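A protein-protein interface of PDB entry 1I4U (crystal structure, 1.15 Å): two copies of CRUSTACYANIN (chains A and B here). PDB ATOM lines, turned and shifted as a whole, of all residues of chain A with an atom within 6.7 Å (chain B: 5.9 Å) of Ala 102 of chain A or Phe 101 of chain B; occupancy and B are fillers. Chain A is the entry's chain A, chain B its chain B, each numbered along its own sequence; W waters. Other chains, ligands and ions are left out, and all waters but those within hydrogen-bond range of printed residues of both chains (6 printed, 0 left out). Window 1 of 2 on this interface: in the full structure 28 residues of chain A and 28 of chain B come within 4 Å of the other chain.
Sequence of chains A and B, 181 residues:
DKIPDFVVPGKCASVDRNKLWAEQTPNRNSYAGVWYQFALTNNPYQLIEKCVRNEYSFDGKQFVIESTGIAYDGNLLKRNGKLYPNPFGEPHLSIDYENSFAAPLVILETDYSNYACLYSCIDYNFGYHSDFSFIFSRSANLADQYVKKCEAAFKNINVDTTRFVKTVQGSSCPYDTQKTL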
ATOM      1  N   TYR A  45       5.404  14.430   2.418  1.00  0.00           N
ATOM      2  CA  TYR A  45       5.490  14.765   3.844  1.00  0.00           C
ATOM      3  C   TYR A  45       4.593  13.878   4.684  1.00  0.00           C
ATOM      4  O   TYR A  45       4.823  13.743   5.874  1.00  0.00           O
ATOM      5  CB  TYR A  45       5.083  16.218   4.061  1.00  0.00           C
ATOM      6  CG  TYR A  45       5.847  17.192   3.217  1.00  0.00           C
ATOM      7  CD1 TYR A  45       7.201  17.435   3.443  1.00  0.00           C
ATOM      8  CD2 TYR A  45       5.250  17.893   2.188  1.00  0.00           C
ATOM      9  CE1 TYR A  45       7.889  18.343   2.660  1.00  0.00           C
ATOM     10  CE2 TYR A  45       5.924  18.798   1.411  1.00  0.00           C
ATOM     11  CZ  TYR A  45       7.258  19.026   1.648  1.00  0.00           C
ATOM     12  OH  TYR A  45       7.920  19.927   0.851  1.00  0.00           O
ATOM     13  N   TYR A  84      -4.297  25.983  13.664  1.00  0.00           N
ATOM     14  CA  TYR A  84      -4.502  27.253  14.370  1.00  0.00           C
ATOM     15  C   TYR A  84      -4.510  28.377  13.359  1.00  0.00           C
ATOM     16  O   TYR A  84      -3.960  28.228  12.249  1.00  0.00           O
ATOM     17  CB  TYR A  84      -3.441  27.477  15.421  1.00  0.00           C
ATOM     18  CG  TYR A  84      -2.012  27.212  15.064  1.00  0.00           C
ATOM     19  CD1 TYR A  84      -1.264  28.137  14.334  1.00  0.00           C
ATOM     20  CD2 TYR A  84      -1.376  26.024  15.427  1.00  0.00           C
ATOM     21  CE1 TYR A  84       0.037  27.877  14.012  1.00  0.00           C
ATOM     22  CE2 TYR A  84      -0.068  25.789  15.091  1.00  0.00           C
ATOM     23  CZ  TYR A  84       0.663  26.700  14.383  1.00  0.00           C
ATOM     24  OH  TYR A  84       1.977  26.515  14.017  1.00  0.00           O
ATOM     25  N   SER A  94      -2.994  27.438   9.772  1.00  0.00           N
ATOM     26  CA  SER A  94      -1.759  26.684   9.681  1.00  0.00           C
ATOM     27  C   SER A  94      -1.960  25.279  10.239  1.00  0.00           C
ATOM     28  O   SER A  94      -2.517  25.133  11.304  1.00  0.00           O
ATOM     29  CB  SER A  94      -0.668  27.313  10.513  1.00  0.00           C
ATOM     30  OG  SER A  94      -0.363  28.623  10.065  1.00  0.00           O
ATOM     31  N   ILE A  95      -1.528  24.288   9.475  1.00  0.00           N
ATOM     32  CA  ILE A  95      -1.529  22.919   9.970  1.00  0.00           C
ATOM     33  C   ILE A  95      -0.085  22.623  10.352  1.00  0.00           C
ATOM     34  O   ILE A  95       0.860  22.851   9.568  1.00  0.00           O
ATOM     35  CB  ILE A  95      -2.054  21.924   8.931  1.00  0.00           C
ATOM     36  CG1 ILE A  95      -2.085  20.513   9.519  1.00  0.00           C
ATOM     37  CG2 ILE A  95      -1.263  21.906   7.632  1.00  0.00           C
ATOM     38  CD1 ILE A  95      -3.211  20.152  10.369  1.00  0.00           C
ATOM     39  N   ASP A  96       0.114  22.160  11.571  1.00  0.00           N
ATOM     40  CA  ASP A  96       1.430  21.956  12.178  1.00  0.00           C
ATOM     41  C   ASP A  96       1.480  20.571  12.803  1.00  0.00           C
ATOM     42  O   ASP A  96       0.483  20.140  13.365  1.00  0.00           O
ATOM     43  CB  ASP A  96       1.671  23.061  13.212  1.00  0.00           C
ATOM     44  CG  ASP A  96       3.111  23.344  13.573  1.00  0.00           C
ATOM     45  OD1 ASP A  96       4.005  22.555  13.206  1.00  0.00           O
ATOM     46  OD2 ASP A  96       3.304  24.384  14.279  1.00  0.00           O
ATOM     47  N   TYR A  97       2.600  19.872  12.714  1.00  0.00           N
ATOM     48  CA  TYR A  97       2.771  18.576  13.303  1.00  0.00           C
ATOM     49  C   TYR A  97       4.074  18.514  14.055  1.00  0.00           C
ATOM     50  O   TYR A  97       5.079  19.151  13.697  1.00  0.00           O
ATOM     51  CB  TYR A  97       2.754  17.432  12.252  1.00  0.00           C
ATOM     52  CG  TYR A  97       1.317  17.050  11.937  1.00  0.00           C
ATOM     53  CD1 TYR A  97       0.525  17.737  11.043  1.00  0.00           C
ATOM     54  CD2 TYR A  97       0.721  15.972  12.561  1.00  0.00           C
ATOM     55  CE1 TYR A  97      -0.803  17.361  10.775  1.00  0.00           C
ATOM     56  CE2 TYR A  97      -0.576  15.584  12.305  1.00  0.00           C
ATOM     57  CZ  TYR A  97      -1.338  16.261  11.412  1.00  0.00           C
ATOM     58  OH  TYR A  97      -2.643  15.903  11.164  1.00  0.00           O
ATOM     59  N   SER A 100       7.965  18.516  12.354  1.00  0.00           N
ATOM     60  CA  SER A 100       7.574  18.800  10.992  1.00  0.00           C
ATOM     61  C   SER A 100       7.570  20.280  10.689  1.00  0.00           C
ATOM     62  O   SER A 100       7.703  21.136  11.560  1.00  0.00           O
ATOM     63  CB  SER A 100       6.189  18.204  10.676  1.00  0.00           C
ATOM     64  OG  SER A 100       6.010  18.238   9.229  1.00  0.00           O
ATOM     65  N   PHE A 101       7.444  20.661   9.424  1.00  0.00           N
ATOM     66  CA  PHE A 101       7.102  22.026   8.997  1.00  0.00           C
ATOM     67  C   PHE A 101       5.610  22.277   9.307  1.00  0.00           C
ATOM     68  O   PHE A 101       4.802  21.373   9.600  1.00  0.00           O
ATOM     69  CB  PHE A 101       7.322  22.215   7.509  1.00  0.00           C
ATOM     70  CG  PHE A 101       8.758  22.440   7.015  1.00  0.00           C
ATOM     71  CD1 PHE A 101       9.903  22.105   7.742  1.00  0.00           C
ATOM     72  CD2 PHE A 101       9.008  23.015   5.770  1.00  0.00           C
ATOM     73  CE1 PHE A 101      11.188  22.324   7.236  1.00  0.00           C
ATOM     74  CE2 PHE A 101      10.272  23.235   5.248  1.00  0.00           C
ATOM     75  CZ  PHE A 101      11.412  22.912   5.989  1.00  0.00           C
ATOM     76  N   ALA A 102       5.167  23.512   9.248  1.00  0.00           N
ATOM     77  CA  ALA A 102       3.785  23.940   9.284  1.00  0.00           C
ATOM     78  C   ALA A 102       3.459  24.552   7.929  1.00  0.00           C
ATOM     79  O   ALA A 102       4.327  25.139   7.287  1.00  0.00           O
ATOM     80  CB  ALA A 102       3.432  24.952  10.387  1.00  0.00           C
ATOM     81  N   ALA A 103       2.194  24.437   7.517  1.00  0.00           N
ATOM     82  CA  ALA A 103       1.813  24.905   6.191  1.00  0.00           C
ATOM     83  C   ALA A 103       0.442  25.521   6.181  1.00  0.00           C
ATOM     84  O   ALA A 103      -0.370  25.179   7.062  1.00  0.00           O
ATOM     85  CB  ALA A 103       1.763  23.732   5.225  1.00  0.00           C
ATOM     86  N   PRO A 104       0.159  26.364   5.207  1.00  0.00           N
ATOM     87  CA  PRO A 104      -1.230  26.828   5.126  1.00  0.00           C
ATOM     88  C   PRO A 104      -2.149  25.664   4.769  1.00  0.00           C
ATOM     89  O   PRO A 104      -1.770  24.754   4.037  1.00  0.00           O
ATOM     90  CB  PRO A 104      -1.217  27.757   3.932  1.00  0.00           C
ATOM     91  CG  PRO A 104      -0.020  27.379   3.145  1.00  0.00           C
ATOM     92  CD  PRO A 104       1.008  26.898   4.157  1.00  0.00           C
ATOM     93  N   SER A 120      -3.377  23.017   0.170  1.00  0.00           N
ATOM     94  CA  SER A 120      -2.203  23.727   0.625  1.00  0.00           C
ATOM     95  C   SER A 120      -1.325  24.045  -0.589  1.00  0.00           C
ATOM     96  O   SER A 120      -1.216  23.198  -1.477  1.00  0.00           O
ATOM     97  CB  SER A 120      -1.396  22.863   1.583  1.00  0.00           C
ATOM     98  OG  SER A 120      -0.330  23.568   2.154  1.00  0.00           O
ATOM     99  N   CYS A 121      -0.718  25.213  -0.619  1.00  0.00           N
ATOM    100  CA  CYS A 121       0.155  25.561  -1.755  1.00  0.00           C
ATOM    101  C   CYS A 121       1.328  26.385  -1.248  1.00  0.00           C
ATOM    102  O   CYS A 121       1.176  27.160  -0.300  1.00  0.00           O
ATOM    103  CB  CYS A 121      -0.635  26.335  -2.816  1.00  0.00           C
ATOM    104  SG  CYS A 121       0.192  26.544  -4.394  1.00  0.00           S
ATOM    105  N   ILE A 122       2.473  26.177  -1.868  1.00  0.00           N
ATOM    106  CA  ILE A 122       3.687  26.940  -1.593  1.00  0.00           C
ATOM    107  C   ILE A 122       4.282  27.426  -2.886  1.00  0.00           C
ATOM    108  O   ILE A 122       4.457  26.593  -3.788  1.00  0.00           O
ATOM    109  CB  ILE A 122       4.681  26.106  -0.780  1.00  0.00           C
ATOM    110  CG1 ILE A 122       5.980  26.786  -0.379  1.00  0.00           C
ATOM    111  CG2 ILE A 122       5.061  24.809  -1.459  1.00  0.00           C
ATOM    112  CD1 ILE A 122       5.828  27.990   0.540  1.00  0.00           C
ATOM    113  N   ASP A 123       4.635  28.715  -2.937  1.00  0.00           N
ATOM    114  CA  ASP A 123       5.416  29.230  -4.040  1.00  0.00           C
ATOM    115  C   ASP A 123       6.915  29.101  -3.808  1.00  0.00           C
ATOM    116  O   ASP A 123       7.451  29.385  -2.743  1.00  0.00           O
ATOM    117  CB  ASP A 123       5.099  30.708  -4.226  1.00  0.00           C
ATOM    118  CG  ASP A 123       3.737  30.905  -4.848  1.00  0.00           C
ATOM    119  OD1 ASP A 123       3.527  30.439  -5.961  1.00  0.00           O
ATOM    120  OD2 ASP A 123       2.925  31.537  -4.176  1.00  0.00           O
ATOM    121  N   SER A 130       4.264  24.193  -5.383  1.00  0.00           N
ATOM    122  CA  SER A 130       3.848  22.865  -5.047  1.00  0.00           C
ATOM    123  C   SER A 130       2.522  22.982  -4.316  1.00  0.00           C
ATOM    124  O   SER A 130       2.348  23.777  -3.421  1.00  0.00           O
ATOM    125  CB  SER A 130       4.804  22.093  -4.160  1.00  0.00           C
ATOM    126  OG  SER A 130       5.880  21.511  -4.914  1.00  0.00           O
ATOM    127  N   PHE A 132      -0.816  20.570  -2.599  1.00  0.00           N
ATOM    128  CA  PHE A 132      -1.135  19.353  -1.870  1.00  0.00           C
ATOM    129  C   PHE A 132      -2.637  19.419  -1.568  1.00  0.00           C
ATOM    130  O   PHE A 132      -3.071  20.344  -0.894  1.00  0.00           O
ATOM    131  CB  PHE A 132      -0.302  19.187  -0.572  1.00  0.00           C
ATOM    132  CG  PHE A 132       1.183  19.216  -0.926  1.00  0.00           C
ATOM    133  CD1 PHE A 132       1.782  18.127  -1.508  1.00  0.00           C
ATOM    134  CD2 PHE A 132       1.932  20.344  -0.749  1.00  0.00           C
ATOM    135  CE1 PHE A 132       3.116  18.196  -1.917  1.00  0.00           C
ATOM    136  CE2 PHE A 132       3.268  20.447  -1.123  1.00  0.00           C
ATOM    137  CZ  PHE A 132       3.840  19.352  -1.746  1.00  0.00           C
ATOM    138  N   TYR B  45      12.918  28.279  -1.300  1.00  0.00           N
ATOM    139  CA  TYR B  45      11.917  29.074  -0.589  1.00  0.00           C
ATOM    140  C   TYR B  45      12.280  30.539  -0.402  1.00  0.00           C
ATOM    141  O   TYR B  45      11.411  31.411  -0.279  1.00  0.00           O
ATOM    142  CB  TYR B  45      11.610  28.486   0.801  1.00  0.00           C
ATOM    143  CG  TYR B  45      11.233  27.025   0.756  1.00  0.00           C
ATOM    144  CD1 TYR B  45      10.003  26.615   0.254  1.00  0.00           C
ATOM    145  CD2 TYR B  45      12.078  26.067   1.208  1.00  0.00           C
ATOM    146  CE1 TYR B  45       9.648  25.291   0.213  1.00  0.00           C
ATOM    147  CE2 TYR B  45      11.756  24.740   1.166  1.00  0.00           C
ATOM    148  CZ  TYR B  45      10.535  24.341   0.669  1.00  0.00           C
ATOM    149  OH  TYR B  45      10.203  23.015   0.625  1.00  0.00           O
ATOM    150  N   ILE B  95      10.483  29.292  12.262  1.00  0.00           N
ATOM    151  CA  ILE B  95      10.623  30.479  11.393  1.00  0.00           C
ATOM    152  C   ILE B  95       9.463  30.500  10.405  1.00  0.00           C
ATOM    153  O   ILE B  95       9.217  29.522   9.703  1.00  0.00           O
ATOM    154  CB  ILE B  95      11.985  30.521  10.703  1.00  0.00           C
ATOM    155  CG1 ILE B  95      12.185  31.840   9.953  1.00  0.00           C
ATOM    156  CG2 ILE B  95      12.246  29.359   9.753  1.00  0.00           C
ATOM    157  CD1 ILE B  95      12.551  32.959  10.853  1.00  0.00           C
ATOM    158  N   ASP B  96       8.716  31.588  10.394  1.00  0.00           N
ATOM    159  CA  ASP B  96       7.462  31.709   9.700  1.00  0.00           C
ATOM    160  C   ASP B  96       7.489  33.004   8.898  1.00  0.00           C
ATOM    161  O   ASP B  96       7.965  33.997   9.420  1.00  0.00           O
ATOM    162  CB  ASP B  96       6.322  31.712  10.726  1.00  0.00           C
ATOM    163  CG  ASP B  96       4.942  31.405  10.192  1.00  0.00           C
ATOM    164  OD1 ASP B  96       4.801  31.382   8.956  1.00  0.00           O
ATOM    165  OD2 ASP B  96       4.023  31.157  11.007  1.00  0.00           O
ATOM    166  N   TYR B  97       7.024  32.996   7.667  1.00  0.00           N
ATOM    167  CA  TYR B  97       6.973  34.188   6.860  1.00  0.00           C
ATOM    168  C   TYR B  97       5.595  34.357   6.245  1.00  0.00           C
ATOM    169  O   TYR B  97       4.897  33.355   6.005  1.00  0.00           O
ATOM    170  CB  TYR B  97       8.047  34.143   5.760  1.00  0.00           C
ATOM    171  CG  TYR B  97       9.375  34.677   6.249  1.00  0.00           C
ATOM    172  CD1 TYR B  97      10.243  33.989   7.086  1.00  0.00           C
ATOM    173  CD2 TYR B  97       9.784  35.939   5.907  1.00  0.00           C
ATOM    174  CE1 TYR B  97      11.423  34.519   7.519  1.00  0.00           C
ATOM    175  CE2 TYR B  97      10.982  36.489   6.324  1.00  0.00           C
ATOM    176  CZ  TYR B  97      11.810  35.770   7.123  1.00  0.00           C
ATOM    177  OH  TYR B  97      13.011  36.282   7.583  1.00  0.00           O
ATOM    178  N   ASN B  99       2.658  34.464   3.794  1.00  0.00           N
ATOM    179  CA  ASN B  99       2.365  33.744   2.563  1.00  0.00           C
ATOM    180  C   ASN B  99       3.458  32.714   2.272  1.00  0.00           C
ATOM    181  O   ASN B  99       3.886  32.585   1.136  1.00  0.00           O
ATOM    182  CB  ASN B  99       2.213  34.681   1.364  1.00  0.00           C
ATOM    183  CG  ASN B  99       1.119  35.702   1.602  1.00  0.00           C
ATOM    184  OD1 ASN B  99       1.372  36.893   1.500  1.00  0.00           O
ATOM    185  ND2 ASN B  99      -0.056  35.230   1.966  1.00  0.00           N
ATOM    186  N   SER B 100       3.884  31.967   3.269  1.00  0.00           N
ATOM    187  CA  SER B 100       4.802  30.845   3.143  1.00  0.00           C
ATOM    188  C   SER B 100       4.466  29.792   4.159  1.00  0.00           C
ATOM    189  O   SER B 100       3.528  29.850   4.999  1.00  0.00           O
ATOM    190  CB  SER B 100       6.237  31.353   3.298  1.00  0.00           C
ATOM    191  OG  SER B 100       7.262  30.418   3.065  1.00  0.00           O
ATOM    192  N   PHE B 101       5.216  28.752   4.203  1.00  0.00           N
ATOM    193  CA  PHE B 101       5.277  27.669   5.170  1.00  0.00           C
ATOM    194  C   PHE B 101       6.097  28.201   6.378  1.00  0.00           C
ATOM    195  O   PHE B 101       6.827  29.202   6.305  1.00  0.00           O
ATOM    196  CB  PHE B 101       5.948  26.405   4.596  1.00  0.00           C
ATOM    197  CG  PHE B 101       5.150  25.463   3.699  1.00  0.00           C
ATOM    198  CD1 PHE B 101       3.983  25.900   3.063  1.00  0.00           C
ATOM    199  CD2 PHE B 101       5.531  24.137   3.479  1.00  0.00           C
ATOM    200  CE1 PHE B 101       3.237  25.043   2.229  1.00  0.00           C
ATOM    201  CE2 PHE B 101       4.824  23.311   2.615  1.00  0.00           C
ATOM    202  CZ  PHE B 101       3.682  23.768   1.984  1.00  0.00           C
ATOM    203  N   ALA B 102       6.012  27.498   7.501  1.00  0.00           N
ATOM    204  CA  ALA B 102       6.879  27.686   8.663  1.00  0.00           C
ATOM    205  C   ALA B 102       7.730  26.444   8.872  1.00  0.00           C
ATOM    206  O   ALA B 102       7.321  25.331   8.576  1.00  0.00           O
ATOM    207  CB  ALA B 102       6.094  27.990   9.919  1.00  0.00           C
ATOM    208  N   ALA B 103       8.936  26.614   9.342  1.00  0.00           N
ATOM    209  CA  ALA B 103       9.870  25.518   9.449  1.00  0.00           C
ATOM    210  C   ALA B 103      10.646  25.567  10.743  1.00  0.00           C
ATOM    211  O   ALA B 103      10.811  26.658  11.306  1.00  0.00           O
ATOM    212  CB  ALA B 103      10.877  25.555   8.322  1.00  0.00           C
HETATM  213  O   HOH W   1       6.647  31.871  -0.778  1.00  0.00           O
HETATM  214  O   HOH W   2      10.521  20.343   1.544  1.00  0.00           O
HETATM  215  O   HOH W   3       2.393  28.992  10.272  1.00  0.00           O
HETATM  216  O   HOH W   4       8.738  30.594  -0.759  1.00  0.00           O
HETATM  217  O   HOH W   5       3.698  30.613  -0.931  1.00  0.00           O
HETATM  218  O   HOH W   6       7.874  22.323  -0.578  1.00  0.00           O
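The backbone NH of Ala 102 of chain A sits at hydrogen-bond distance from the backbone carbonyl oxygen of Ala 102 of chain B (2.9 Å).
The backbone carbonyl oxygen (O) of Ser 120 of chain A is in hydrogen-bond range of the backbone NH (N) of Phe 132 of chain A, 2.9 Å away. The backbone NH of Ile 95 of chain A is in hydrogen-bond range of the backbone carbonyl oxygen of Ala 103 of chain A (2.8 Å). The backbone carbonyl oxygen of Pro 104 of chain A sits at hydrogen-bond distance from the side-chain hydroxyl of Ser 120 of chain A (2.7 Å). N of Ile 95 of chain B sits at hydrogen-bond distance from O of Ala 103 of chain B, at 2.8 Å. The backbone carbonyl oxygen of Ser 130 of chain A sits at hydrogen-bond distance from the backbone NH of Ile 122 of chain A (2.9 Å).
Among the printed residues, merely in contact across the chains: Phe 101 of chain A with Ala 102 of chain B (3.3 Å), Pro 104 of chain A with Phe 101 of chain B (3.3 Å), Ala 102 of chain A with Phe 101 of chain B (3.4 Å), Phe 101 of chain A with Ala 103 of chain B (3.4 Å), Ile 122 of chain A with Phe 101 of chain B (3.5 Å), Ala 103 of chain A with Phe 101 of chain B (3.6 Å), Ile 122 of chain A with Ser 100 of chain B (3.8 Å), Tyr 45 of chain A with Tyr 45 of chain B (3.8 Å), Ser 120 of chain A with Phe 101 of chain B (3.9 Å), Cys 121 of chain A with Phe 101 of chain B (3.9 Å) and Pro 104 of chain A with Ser 100 of chain B (3.97 Å).
Of the printed residues of chain A, Ser 100 of chain B touches Pro 104 (3.97 Å) and Ile 122 (3.8 Å). Phe 101 of chain B touches just these residues of chain A: Ala 102, Ala 103, Pro 104, Ser 120, Cys 121 and Ile 122. Of the printed residues of chain A, Ala 103 of chain B touches Phe 101 (3.4 Å). The nearest residue of chain B that does not touch Ala 102 of chain A is Ala 103 of chain B (4.9 Å).
Hydrophobic or aromatic side chains of chain A within 4 Å of the printed part of chain B: Tyr 45, Phe 101, Ala 103, Pro 104 and Ile 122. Of the 9 printed residues of chain B, 5 touch a printed residue of chain A. Printed residues of chain B that touch a printed residue of chain A: Tyr 45, Ser 100, Phe 101, Ala 102 and Ala 103.
Tyr 45 of chain A touches its own counterpart, Tyr 45 of chain B. Phe 101 of chain A touches Ala 102 of chain B, and with the chains exchanged Ala 102 of chain A touches Phe 101 of chain B. Phe 101 of chain A touches Ala 103 of chain B, and with the chains exchanged Ala 103 of chain A touches Phe 101 of chain B. Ala 102 of chain B touches its own counterpart, Ala 102 of chain A. Positions printed for both chains: 45, 95, 96, 97, 100, 101, 102 and 103. Of the 12 pairs that touch across the chains among the printed residues, 6 have their exchanged pair printed and touching as well.
Water W4 lies within hydrogen-bond range of the backbone carbonyl oxygen of Asp 123 of chain A (2.7 Å) and the backbone carbonyl oxygen of Tyr 45 of chain B (2.8 Å). Water W6 bridges the side-chain hydroxyl (OH) of Tyr 45 of chain B and the side-chain hydroxyl (OH) of Tyr 45 of chain A. Water W2 bridges OH of Tyr 45 of chain A and OH of Tyr 45 of chain B. Water W3 lies within hydrogen-bond range of the side-chain hydroxyl (OG) of Ser 94 of chain A and the side-chain carboxylate (OD2) of Asp 96 of chain B. Water W5 lies within hydrogen-bond range of O of Asn 99 of chain B (2.9 Å) and N of Asp 123 of chain A (2.9 Å). Water W1 lies within hydrogen-bond range of O of Asp 123 of chain A and O of Asn 99 of chain B.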
